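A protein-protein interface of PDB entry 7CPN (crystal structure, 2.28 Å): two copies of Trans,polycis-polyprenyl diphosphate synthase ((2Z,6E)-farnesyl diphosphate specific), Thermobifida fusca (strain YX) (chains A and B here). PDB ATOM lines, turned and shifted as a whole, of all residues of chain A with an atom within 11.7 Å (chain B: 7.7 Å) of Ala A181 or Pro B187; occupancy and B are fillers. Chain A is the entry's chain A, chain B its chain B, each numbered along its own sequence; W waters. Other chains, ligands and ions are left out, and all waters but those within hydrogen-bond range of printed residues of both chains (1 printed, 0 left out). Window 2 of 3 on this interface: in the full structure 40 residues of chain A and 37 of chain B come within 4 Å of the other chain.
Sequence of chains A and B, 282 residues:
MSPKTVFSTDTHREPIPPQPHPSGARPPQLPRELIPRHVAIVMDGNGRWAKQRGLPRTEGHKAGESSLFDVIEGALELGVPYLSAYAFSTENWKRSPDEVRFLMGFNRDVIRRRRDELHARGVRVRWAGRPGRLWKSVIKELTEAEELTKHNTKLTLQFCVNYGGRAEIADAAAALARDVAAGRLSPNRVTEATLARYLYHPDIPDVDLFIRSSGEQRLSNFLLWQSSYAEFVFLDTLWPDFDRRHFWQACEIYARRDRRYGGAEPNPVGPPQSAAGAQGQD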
ATOM      1  N   ARG A 130      26.311  33.608 -10.904  1.00  0.00           N
ATOM      2  CA  ARG A 130      25.856  32.203 -10.975  1.00  0.00           C
ATOM      3  C   ARG A 130      24.906  31.927  -9.826  1.00  0.00           C
ATOM      4  O   ARG A 130      25.140  32.429  -8.715  1.00  0.00           O
ATOM      5  CB  ARG A 130      27.040  31.246 -10.817  1.00  0.00           C
ATOM      6  CG  ARG A 130      27.901  31.108 -12.050  1.00  0.00           C
ATOM      7  CD  ARG A 130      29.083  30.213 -11.701  1.00  0.00           C
ATOM      8  NE  ARG A 130      29.821  29.855 -12.902  1.00  0.00           N
ATOM      9  CZ  ARG A 130      31.009  29.243 -12.913  1.00  0.00           C
ATOM     10  NH1 ARG A 130      31.635  28.974 -11.787  1.00  0.00           N
ATOM     11  NH2 ARG A 130      31.600  28.967 -14.058  1.00  0.00           N
ATOM     12  N   ALA A 167      34.668  32.889 -14.313  1.00  0.00           N
ATOM     13  CA  ALA A 167      33.409  32.105 -14.277  1.00  0.00           C
ATOM     14  C   ALA A 167      32.476  32.551 -15.413  1.00  0.00           C
ATOM     15  O   ALA A 167      31.889  31.685 -16.068  1.00  0.00           O
ATOM     16  CB  ALA A 167      32.739  32.246 -12.944  1.00  0.00           C
ATOM     17  N   ILE A 169      33.268  33.979 -18.352  1.00  0.00           N
ATOM     18  CA  ILE A 169      33.873  33.528 -19.637  1.00  0.00           C
ATOM     19  C   ILE A 169      33.687  32.010 -19.811  1.00  0.00           C
ATOM     20  O   ILE A 169      33.385  31.565 -20.938  1.00  0.00           O
ATOM     21  CB  ILE A 169      35.345  33.959 -19.678  1.00  0.00           C
ATOM     22  CG1 ILE A 169      35.442  35.488 -19.729  1.00  0.00           C
ATOM     23  CG2 ILE A 169      36.064  33.309 -20.850  1.00  0.00           C
ATOM     24  CD1 ILE A 169      36.795  36.022 -19.470  1.00  0.00           C
ATOM     25  N   ALA A 170      33.873  31.238 -18.740  1.00  0.00           N
ATOM     26  CA  ALA A 170      33.684  29.774 -18.760  1.00  0.00           C
ATOM     27  C   ALA A 170      32.221  29.442 -19.033  1.00  0.00           C
ATOM     28  O   ALA A 170      31.978  28.555 -19.841  1.00  0.00           O
ATOM     29  CB  ALA A 170      34.191  29.141 -17.504  1.00  0.00           C
ATOM     30  N   ASP A 171      31.284  30.148 -18.414  1.00  0.00           N
ATOM     31  CA  ASP A 171      29.831  29.977 -18.655  1.00  0.00           C
ATOM     32  C   ASP A 171      29.488  30.385 -20.084  1.00  0.00           C
ATOM     33  O   ASP A 171      28.593  29.771 -20.670  1.00  0.00           O
ATOM     34  CB  ASP A 171      29.010  30.763 -17.647  1.00  0.00           C
ATOM     35  CG  ASP A 171      29.078  30.188 -16.233  1.00  0.00           C
ATOM     36  OD1 ASP A 171      29.655  29.107 -16.066  1.00  0.00           O
ATOM     37  OD2 ASP A 171      28.573  30.862 -15.300  1.00  0.00           O
ATOM     38  N   ALA A 172      30.156  31.383 -20.647  1.00  0.00           N
ATOM     39  CA  ALA A 172      29.990  31.747 -22.073  1.00  0.00           C
ATOM     40  C   ALA A 172      30.463  30.582 -22.952  1.00  0.00           C
ATOM     41  O   ALA A 172      29.767  30.269 -23.927  1.00  0.00           O
ATOM     42  CB  ALA A 172      30.716  33.029 -22.421  1.00  0.00           C
ATOM     43  N   ALA A 173      31.657  30.035 -22.683  1.00  0.00           N
ATOM     44  CA  ALA A 173      32.201  28.903 -23.456  1.00  0.00           C
ATOM     45  C   ALA A 173      31.272  27.665 -23.336  1.00  0.00           C
ATOM     46  O   ALA A 173      31.074  26.972 -24.345  1.00  0.00           O
ATOM     47  CB  ALA A 173      33.605  28.595 -23.040  1.00  0.00           C
ATOM     48  N   ALA A 174      30.740  27.380 -22.151  1.00  0.00           N
ATOM     49  CA  ALA A 174      29.791  26.280 -21.893  1.00  0.00           C
ATOM     50  C   ALA A 174      28.541  26.451 -22.751  1.00  0.00           C
ATOM     51  O   ALA A 174      28.152  25.486 -23.405  1.00  0.00           O
ATOM     52  CB  ALA A 174      29.450  26.182 -20.419  1.00  0.00           C
ATOM     53  N   ALA A 175      27.934  27.633 -22.752  1.00  0.00           N
ATOM     54  CA  ALA A 175      26.710  27.925 -23.522  1.00  0.00           C
ATOM     55  C   ALA A 175      27.025  27.816 -25.017  1.00  0.00           C
ATOM     56  O   ALA A 175      26.214  27.257 -25.743  1.00  0.00           O
ATOM     57  CB  ALA A 175      26.143  29.277 -23.186  1.00  0.00           C
ATOM     58  N   LEU A 176      28.160  28.327 -25.454  1.00  0.00           N
ATOM     59  CA  LEU A 176      28.625  28.146 -26.849  1.00  0.00           C
ATOM     60  C   LEU A 176      28.771  26.650 -27.154  1.00  0.00           C
ATOM     61  O   LEU A 176      28.290  26.209 -28.230  1.00  0.00           O
ATOM     62  CB  LEU A 176      29.919  28.912 -27.036  1.00  0.00           C
ATOM     63  CG  LEU A 176      30.386  29.003 -28.491  1.00  0.00           C
ATOM     64  CD1 LEU A 176      31.166  30.298 -28.709  1.00  0.00           C
ATOM     65  CD2 LEU A 176      31.237  27.808 -28.903  1.00  0.00           C
ATOM     66  N   ALA A 177      29.399  25.907 -26.254  1.00  0.00           N
ATOM     67  CA  ALA A 177      29.586  24.437 -26.391  1.00  0.00           C
ATOM     68  C   ALA A 177      28.226  23.723 -26.571  1.00  0.00           C
ATOM     69  O   ALA A 177      28.138  22.844 -27.433  1.00  0.00           O
ATOM     70  CB  ALA A 177      30.349  23.887 -25.207  1.00  0.00           C
ATOM     71  N   ARG A 178      27.211  24.100 -25.797  1.00  0.00           N
ATOM     72  CA  ARG A 178      25.851  23.495 -25.871  1.00  0.00           C
ATOM     73  C   ARG A 178      25.239  23.754 -27.250  1.00  0.00           C
ATOM     74  O   ARG A 178      24.657  22.814 -27.808  1.00  0.00           O
ATOM     75  CB  ARG A 178      24.921  24.000 -24.773  1.00  0.00           C
ATOM     76  CG  ARG A 178      25.239  23.422 -23.400  1.00  0.00           C
ATOM     77  CD  ARG A 178      24.267  23.895 -22.327  1.00  0.00           C
ATOM     78  NE  ARG A 178      24.968  24.519 -21.208  1.00  0.00           N
ATOM     79  CZ  ARG A 178      24.981  25.823 -20.917  1.00  0.00           C
ATOM     80  NH1 ARG A 178      24.311  26.714 -21.635  1.00  0.00           N
ATOM     81  NH2 ARG A 178      25.669  26.236 -19.873  1.00  0.00           N
ATOM     82  N   ASP A 179      25.392  24.960 -27.792  1.00  0.00           N
ATOM     83  CA  ASP A 179      24.883  25.302 -29.144  1.00  0.00           C
ATOM     84  C   ASP A 179      25.629  24.457 -30.181  1.00  0.00           C
ATOM     85  O   ASP A 179      24.986  24.023 -31.156  1.00  0.00           O
ATOM     86  CB  ASP A 179      24.968  26.802 -29.416  1.00  0.00           C
ATOM     87  CG  ASP A 179      23.838  27.596 -28.817  1.00  0.00           C
ATOM     88  OD1 ASP A 179      22.972  26.962 -28.187  1.00  0.00           O
ATOM     89  OD2 ASP A 179      23.844  28.837 -28.974  1.00  0.00           O
ATOM     90  N   VAL A 180      26.921  24.206 -29.976  1.00  0.00           N
ATOM     91  CA  VAL A 180      27.711  23.380 -30.926  1.00  0.00           C
ATOM     92  C   VAL A 180      27.225  21.924 -30.864  1.00  0.00           C
ATOM     93  O   VAL A 180      27.024  21.351 -31.933  1.00  0.00           O
ATOM     94  CB  VAL A 180      29.227  23.516 -30.697  1.00  0.00           C
ATOM     95  CG1 VAL A 180      29.990  22.445 -31.481  1.00  0.00           C
ATOM     96  CG2 VAL A 180      29.700  24.909 -31.118  1.00  0.00           C
ATOM     97  N   ALA A 181      27.006  21.372 -29.672  1.00  0.00           N
ATOM     98  CA  ALA A 181      26.580  19.966 -29.453  1.00  0.00           C
ATOM     99  C   ALA A 181      25.196  19.747 -30.085  1.00  0.00           C
ATOM    100  O   ALA A 181      24.984  18.689 -30.684  1.00  0.00           O
ATOM    101  CB  ALA A 181      26.564  19.627 -27.977  1.00  0.00           C
ATOM    102  N   ALA A 182      24.308  20.728 -29.974  1.00  0.00           N
ATOM    103  CA  ALA A 182      22.930  20.684 -30.525  1.00  0.00           C
ATOM    104  C   ALA A 182      22.949  20.960 -32.031  1.00  0.00           C
ATOM    105  O   ALA A 182      21.894  20.818 -32.641  1.00  0.00           O
ATOM    106  CB  ALA A 182      22.039  21.679 -29.804  1.00  0.00           C
ATOM    107  N   GLY A 183      24.096  21.322 -32.616  1.00  0.00           N
ATOM    108  CA  GLY A 183      24.198  21.604 -34.059  1.00  0.00           C
ATOM    109  C   GLY A 183      23.550  22.926 -34.461  1.00  0.00           C
ATOM    110  O   GLY A 183      23.297  23.104 -35.666  1.00  0.00           O
ATOM    111  N   ARG A 184      23.343  23.854 -33.523  1.00  0.00           N
ATOM    112  CA  ARG A 184      22.829  25.228 -33.814  1.00  0.00           C
ATOM    113  C   ARG A 184      23.969  26.138 -34.279  1.00  0.00           C
ATOM    114  O   ARG A 184      23.691  27.236 -34.814  1.00  0.00           O
ATOM    115  CB  ARG A 184      22.148  25.841 -32.581  1.00  0.00           C
ATOM    116  CG  ARG A 184      20.840  25.158 -32.221  1.00  0.00           C
ATOM    117  CD  ARG A 184      20.095  25.852 -31.083  1.00  0.00           C
ATOM    118  NE  ARG A 184      20.708  25.597 -29.796  1.00  0.00           N
ATOM    119  CZ  ARG A 184      20.375  24.643 -28.935  1.00  0.00           C
ATOM    120  NH1 ARG A 184      19.384  23.807 -29.181  1.00  0.00           N
ATOM    121  NH2 ARG A 184      21.048  24.528 -27.811  1.00  0.00           N
ATOM    122  N   LEU A 185      25.222  25.723 -34.083  1.00  0.00           N
ATOM    123  CA  LEU A 185      26.407  26.593 -34.307  1.00  0.00           C
ATOM    124  C   LEU A 185      27.573  25.728 -34.781  1.00  0.00           C
ATOM    125  O   LEU A 185      27.783  24.661 -34.167  1.00  0.00           O
ATOM    126  CB  LEU A 185      26.745  27.281 -32.972  1.00  0.00           C
ATOM    127  CG  LEU A 185      27.913  28.247 -32.977  1.00  0.00           C
ATOM    128  CD1 LEU A 185      27.576  29.434 -33.832  1.00  0.00           C
ATOM    129  CD2 LEU A 185      28.321  28.673 -31.573  1.00  0.00           C
ATOM    130  N   SER A 186      28.332  26.185 -35.774  1.00  0.00           N
ATOM    131  CA  SER A 186      29.596  25.549 -36.213  1.00  0.00           C
ATOM    132  C   SER A 186      30.737  25.798 -35.229  1.00  0.00           C
ATOM    133  O   SER A 186      30.932  26.917 -34.783  1.00  0.00           O
ATOM    134  CB  SER A 186      29.996  26.060 -37.550  1.00  0.00           C
ATOM    135  OG  SER A 186      31.314  25.619 -37.862  1.00  0.00           O
ATOM    136  N   PRO A 187      31.558  24.779 -34.901  1.00  0.00           N
ATOM    137  CA  PRO A 187      32.707  24.998 -34.021  1.00  0.00           C
ATOM    138  C   PRO A 187      33.843  25.763 -34.732  1.00  0.00           C
ATOM    139  O   PRO A 187      34.737  26.229 -34.034  1.00  0.00           O
ATOM    140  CB  PRO A 187      33.124  23.585 -33.598  1.00  0.00           C
ATOM    141  CG  PRO A 187      32.643  22.706 -34.730  1.00  0.00           C
ATOM    142  CD  PRO A 187      31.402  23.374 -35.310  1.00  0.00           C
ATOM    143  N   ASN A 188      33.806  25.843 -36.071  1.00  0.00           N
ATOM    144  CA  ASN A 188      35.010  26.187 -36.882  1.00  0.00           C
ATOM    145  C   ASN A 188      35.093  27.700 -37.081  1.00  0.00           C
ATOM    146  O   ASN A 188      36.170  28.146 -37.518  1.00  0.00           O
ATOM    147  CB  ASN A 188      35.069  25.445 -38.224  1.00  0.00           C
ATOM    148  CG  ASN A 188      35.169  23.946 -38.040  1.00  0.00           C
ATOM    149  OD1 ASN A 188      36.031  23.453 -37.314  1.00  0.00           O
ATOM    150  ND2 ASN A 188      34.261  23.215 -38.662  1.00  0.00           N
ATOM    151  N   VAL A 190      34.400  30.242 -34.594  1.00  0.00           N
ATOM    152  CA  VAL A 190      34.225  30.921 -33.268  1.00  0.00           C
ATOM    153  C   VAL A 190      35.212  32.085 -33.198  1.00  0.00           C
ATOM    154  O   VAL A 190      36.393  31.838 -33.280  1.00  0.00           O
ATOM    155  CB  VAL A 190      34.339  29.966 -32.068  1.00  0.00           C
ATOM    156  CG1 VAL A 190      34.315  30.715 -30.754  1.00  0.00           C
ATOM    157  CG2 VAL A 190      33.223  28.929 -32.092  1.00  0.00           C
ATOM    158  N   TYR A 198      27.646  35.333 -25.681  1.00  0.00           N
ATOM    159  CA  TYR A 198      27.271  34.367 -24.611  1.00  0.00           C
ATOM    160  C   TYR A 198      27.669  34.872 -23.219  1.00  0.00           C
ATOM    161  O   TYR A 198      27.492  34.093 -22.244  1.00  0.00           O
ATOM    162  CB  TYR A 198      27.870  32.992 -24.892  1.00  0.00           C
ATOM    163  CG  TYR A 198      27.348  32.313 -26.130  1.00  0.00           C
ATOM    164  CD1 TYR A 198      27.924  32.513 -27.374  1.00  0.00           C
ATOM    165  CD2 TYR A 198      26.240  31.470 -26.055  1.00  0.00           C
ATOM    166  CE1 TYR A 198      27.439  31.861 -28.505  1.00  0.00           C
ATOM    167  CE2 TYR A 198      25.740  30.825 -27.174  1.00  0.00           C
ATOM    168  CZ  TYR A 198      26.360  30.988 -28.396  1.00  0.00           C
ATOM    169  OH  TYR A 198      25.846  30.330 -29.482  1.00  0.00           O
ATOM    170  N   LEU B 176      38.088  24.336 -27.856  1.00  0.00           N
ATOM    171  CA  LEU B 176      37.164  23.593 -26.969  1.00  0.00           C
ATOM    172  C   LEU B 176      35.926  23.174 -27.776  1.00  0.00           C
ATOM    173  O   LEU B 176      35.503  22.024 -27.620  1.00  0.00           O
ATOM    174  CB  LEU B 176      36.800  24.501 -25.808  1.00  0.00           C
ATOM    175  CG  LEU B 176      35.973  23.879 -24.704  1.00  0.00           C
ATOM    176  CD1 LEU B 176      36.305  24.577 -23.386  1.00  0.00           C
ATOM    177  CD2 LEU B 176      34.486  23.982 -25.013  1.00  0.00           C
ATOM    178  N   ALA B 177      35.354  24.071 -28.582  1.00  0.00           N
ATOM    179  CA  ALA B 177      34.154  23.805 -29.408  1.00  0.00           C
ATOM    180  C   ALA B 177      34.437  22.619 -30.356  1.00  0.00           C
ATOM    181  O   ALA B 177      33.554  21.754 -30.489  1.00  0.00           O
ATOM    182  CB  ALA B 177      33.739  25.036 -30.169  1.00  0.00           C
ATOM    183  N   VAL B 180      34.319  19.459 -28.510  1.00  0.00           N
ATOM    184  CA  VAL B 180      32.900  19.129 -28.193  1.00  0.00           C
ATOM    185  C   VAL B 180      32.244  18.492 -29.431  1.00  0.00           C
ATOM    186  O   VAL B 180      31.588  17.450 -29.258  1.00  0.00           O
ATOM    187  CB  VAL B 180      32.116  20.342 -27.670  1.00  0.00           C
ATOM    188  CG1 VAL B 180      30.627  20.100 -27.699  1.00  0.00           C
ATOM    189  CG2 VAL B 180      32.578  20.727 -26.277  1.00  0.00           C
ATOM    190  N   ALA B 181      32.441  19.056 -30.630  1.00  0.00           N
ATOM    191  CA  ALA B 181      31.811  18.578 -31.882  1.00  0.00           C
ATOM    192  C   ALA B 181      32.302  17.147 -32.190  1.00  0.00           C
ATOM    193  O   ALA B 181      31.520  16.342 -32.644  1.00  0.00           O
ATOM    194  CB  ALA B 181      32.119  19.518 -33.012  1.00  0.00           C
ATOM    195  N   GLY B 183      33.179  15.019 -30.006  1.00  0.00           N
ATOM    196  CA  GLY B 183      32.763  14.137 -28.902  1.00  0.00           C
ATOM    197  C   GLY B 183      33.889  13.766 -27.950  1.00  0.00           C
ATOM    198  O   GLY B 183      33.690  12.828 -27.169  1.00  0.00           O
ATOM    199  N   LEU B 185      34.805  15.866 -25.635  1.00  0.00           N
ATOM    200  CA  LEU B 185      34.480  16.699 -24.455  1.00  0.00           C
ATOM    201  C   LEU B 185      32.974  16.886 -24.347  1.00  0.00           C
ATOM    202  O   LEU B 185      32.366  17.214 -25.355  1.00  0.00           O
ATOM    203  CB  LEU B 185      35.194  18.055 -24.621  1.00  0.00           C
ATOM    204  CG  LEU B 185      35.067  18.998 -23.429  1.00  0.00           C
ATOM    205  CD1 LEU B 185      35.743  18.391 -22.196  1.00  0.00           C
ATOM    206  CD2 LEU B 185      35.706  20.331 -23.753  1.00  0.00           C
ATOM    207  N   SER B 186      32.403  16.711 -23.159  1.00  0.00           N
ATOM    208  CA  SER B 186      30.964  16.957 -22.898  1.00  0.00           C
ATOM    209  C   SER B 186      30.738  18.450 -22.695  1.00  0.00           C
ATOM    210  O   SER B 186      31.508  19.082 -21.969  1.00  0.00           O
ATOM    211  CB  SER B 186      30.473  16.220 -21.696  1.00  0.00           C
ATOM    212  OG  SER B 186      29.193  16.720 -21.327  1.00  0.00           O
ATOM    213  N   PRO B 187      29.662  19.043 -23.272  1.00  0.00           N
ATOM    214  CA  PRO B 187      29.373  20.452 -23.073  1.00  0.00           C
ATOM    215  C   PRO B 187      28.905  20.769 -21.654  1.00  0.00           C
ATOM    216  O   PRO B 187      28.924  21.939 -21.278  1.00  0.00           O
ATOM    217  CB  PRO B 187      28.277  20.756 -24.106  1.00  0.00           C
ATOM    218  CG  PRO B 187      27.618  19.435 -24.360  1.00  0.00           C
ATOM    219  CD  PRO B 187      28.713  18.404 -24.196  1.00  0.00           C
ATOM    220  N   ASN B 188      28.546  19.746 -20.876  1.00  0.00           N
ATOM    221  CA  ASN B 188      28.018  19.923 -19.491  1.00  0.00           C
ATOM    222  C   ASN B 188      29.169  19.947 -18.490  1.00  0.00           C
ATOM    223  O   ASN B 188      28.911  20.262 -17.344  1.00  0.00           O
ATOM    224  CB  ASN B 188      26.957  18.875 -19.150  1.00  0.00           C
ATOM    225  CG  ASN B 188      25.714  19.048 -20.008  1.00  0.00           C
ATOM    226  OD1 ASN B 188      25.429  18.205 -20.858  1.00  0.00           O
ATOM    227  ND2 ASN B 188      25.016  20.168 -19.851  1.00  0.00           N
ATOM    228  N   ARG B 189      30.398  19.694 -18.927  1.00  0.00           N
ATOM    229  CA  ARG B 189      31.616  19.771 -18.076  1.00  0.00           C
ATOM    230  C   ARG B 189      32.570  20.865 -18.597  1.00  0.00           C
ATOM    231  O   ARG B 189      33.794  20.688 -18.479  1.00  0.00           O
ATOM    232  CB  ARG B 189      32.251  18.372 -18.050  1.00  0.00           C
ATOM    233  N   VAL B 190      32.063  21.955 -19.180  1.00  0.00           N
ATOM    234  CA  VAL B 190      32.925  23.100 -19.616  1.00  0.00           C
ATOM    235  C   VAL B 190      33.005  24.078 -18.445  1.00  0.00           C
ATOM    236  O   VAL B 190      32.004  24.654 -18.107  1.00  0.00           O
ATOM    237  CB  VAL B 190      32.455  23.786 -20.911  1.00  0.00           C
ATOM    238  CG1 VAL B 190      33.305  25.008 -21.210  1.00  0.00           C
ATOM    239  CG2 VAL B 190      32.485  22.808 -22.075  1.00  0.00           C
ATOM    240  N   THR B 191      34.162  24.151 -17.802  1.00  0.00           N
ATOM    241  CA  THR B 191      34.434  24.923 -16.572  1.00  0.00           C
ATOM    242  C   THR B 191      35.642  25.803 -16.857  1.00  0.00           C
ATOM    243  O   THR B 191      36.257  25.644 -17.913  1.00  0.00           O
ATOM    244  CB  THR B 191      34.737  23.986 -15.381  1.00  0.00           C
ATOM    245  OG1 THR B 191      35.918  23.239 -15.727  1.00  0.00           O
ATOM    246  CG2 THR B 191      33.551  23.095 -15.054  1.00  0.00           C
HETATM  247  O   HOH W   1      31.240  26.890 -16.595  1.00  0.00           O
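Among the printed residues, merely in contact across the chains: Ala A174 with Val B190 (3.6 Å), Pro A187 with Ala B177 (3.6 Å), Pro A187 with Ala B181 (3.7 Å), Ala A170 with Thr B191 (3.7 Å), Ala A177 with Val B180 (3.7 Å), Val A180 with Ala B177 (3.8 Å), Ala A181 with Pro B187 (3.8 Å), Ala A177 with Pro B187 (3.9 Å), Arg A178 with Pro B187 (3.9 Å), Val A180 with Ala B181 (3.9 Å), Ala A177 with Val B190 (3.9 Å), Leu A176 with Ala B177 (3.9 Å) and Ala A173 with Val B190 (3.96 Å).
Ala A181 touches just one residue of chain B: Pro B187. Of chain A, only Ala A177, Arg A178 and Ala A181 come within 4 Å of Pro B187. Val B180 touches just one residue of chain A: Ala A177. Ala B181 touches just these residues of chain A: Val A180 (3.9 Å) and Pro A187 (3.7 Å). No residue of chain A comes within 4 Å of Leu B185. Val B190 touches three residues of chain A. Of the printed residues of chain A, Ala B177 touches Leu A176, Val A180 and Pro A187. Of the printed residues of chain B, Leu A176 touches Ala B177. Printed residues of chain B within 4 Å of Val A180: Ala B177 and Ala B181. Printed residues of chain B within 4 Å of Pro A187: Ala B177 and Ala B181. Ala A172 touches none of the printed residues of chain B. Val A190 touches none of the printed residues of chain B. The nearest residue of chain B that does not touch Ala A181 is Val B180 (4.1 Å).
Of the 12 printed residues of chain B, 6 touch a printed residue of chain A. Printed residues of chain B that touch a printed residue of chain A: Ala B177, Val B180, Ala B181, Pro B187, Val B190 and Thr B191. Along chain B the printed residues that touch a printed residue of chain A span positions 177 to 191. Of the 24 printed residues of chain A, 9 touch a printed residue of chain B. Hydrophobic or aromatic side chains of chain A within 4 Å of the printed part of chain B: Ala A170, Ala A174, Leu A176, Ala A177, Val A180, Ala A181 and Pro A187.
Ala A177 touches Val B180, and with the chains exchanged Val A180 touches Ala B177. Ala A177 touches Val B190, but with the chains exchanged Val A190 does not touch Ala B177 (4.4 Å). Val A180 touches Ala B181, but with the chains exchanged Ala A181 does not touch Val B180 (4.1 Å). Ala A181 touches Pro B187, and with the chains exchanged Pro A187 touches Ala B181. Positions printed for both chains: 176, 177, 180, 181, 183, 185, 186, 187, 188 and 190. Of the 13 pairs that touch across the chains among the printed residues, 6 have their exchanged pair printed and touching as well.
Water W1 lies within hydrogen-bond range of the side-chain carboxylate of Asp A171 (2.8 Å), the backbone carbonyl oxygen of Val B190 (2.8 Å) and the guanidinium group of Arg A130 (3.3 Å).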
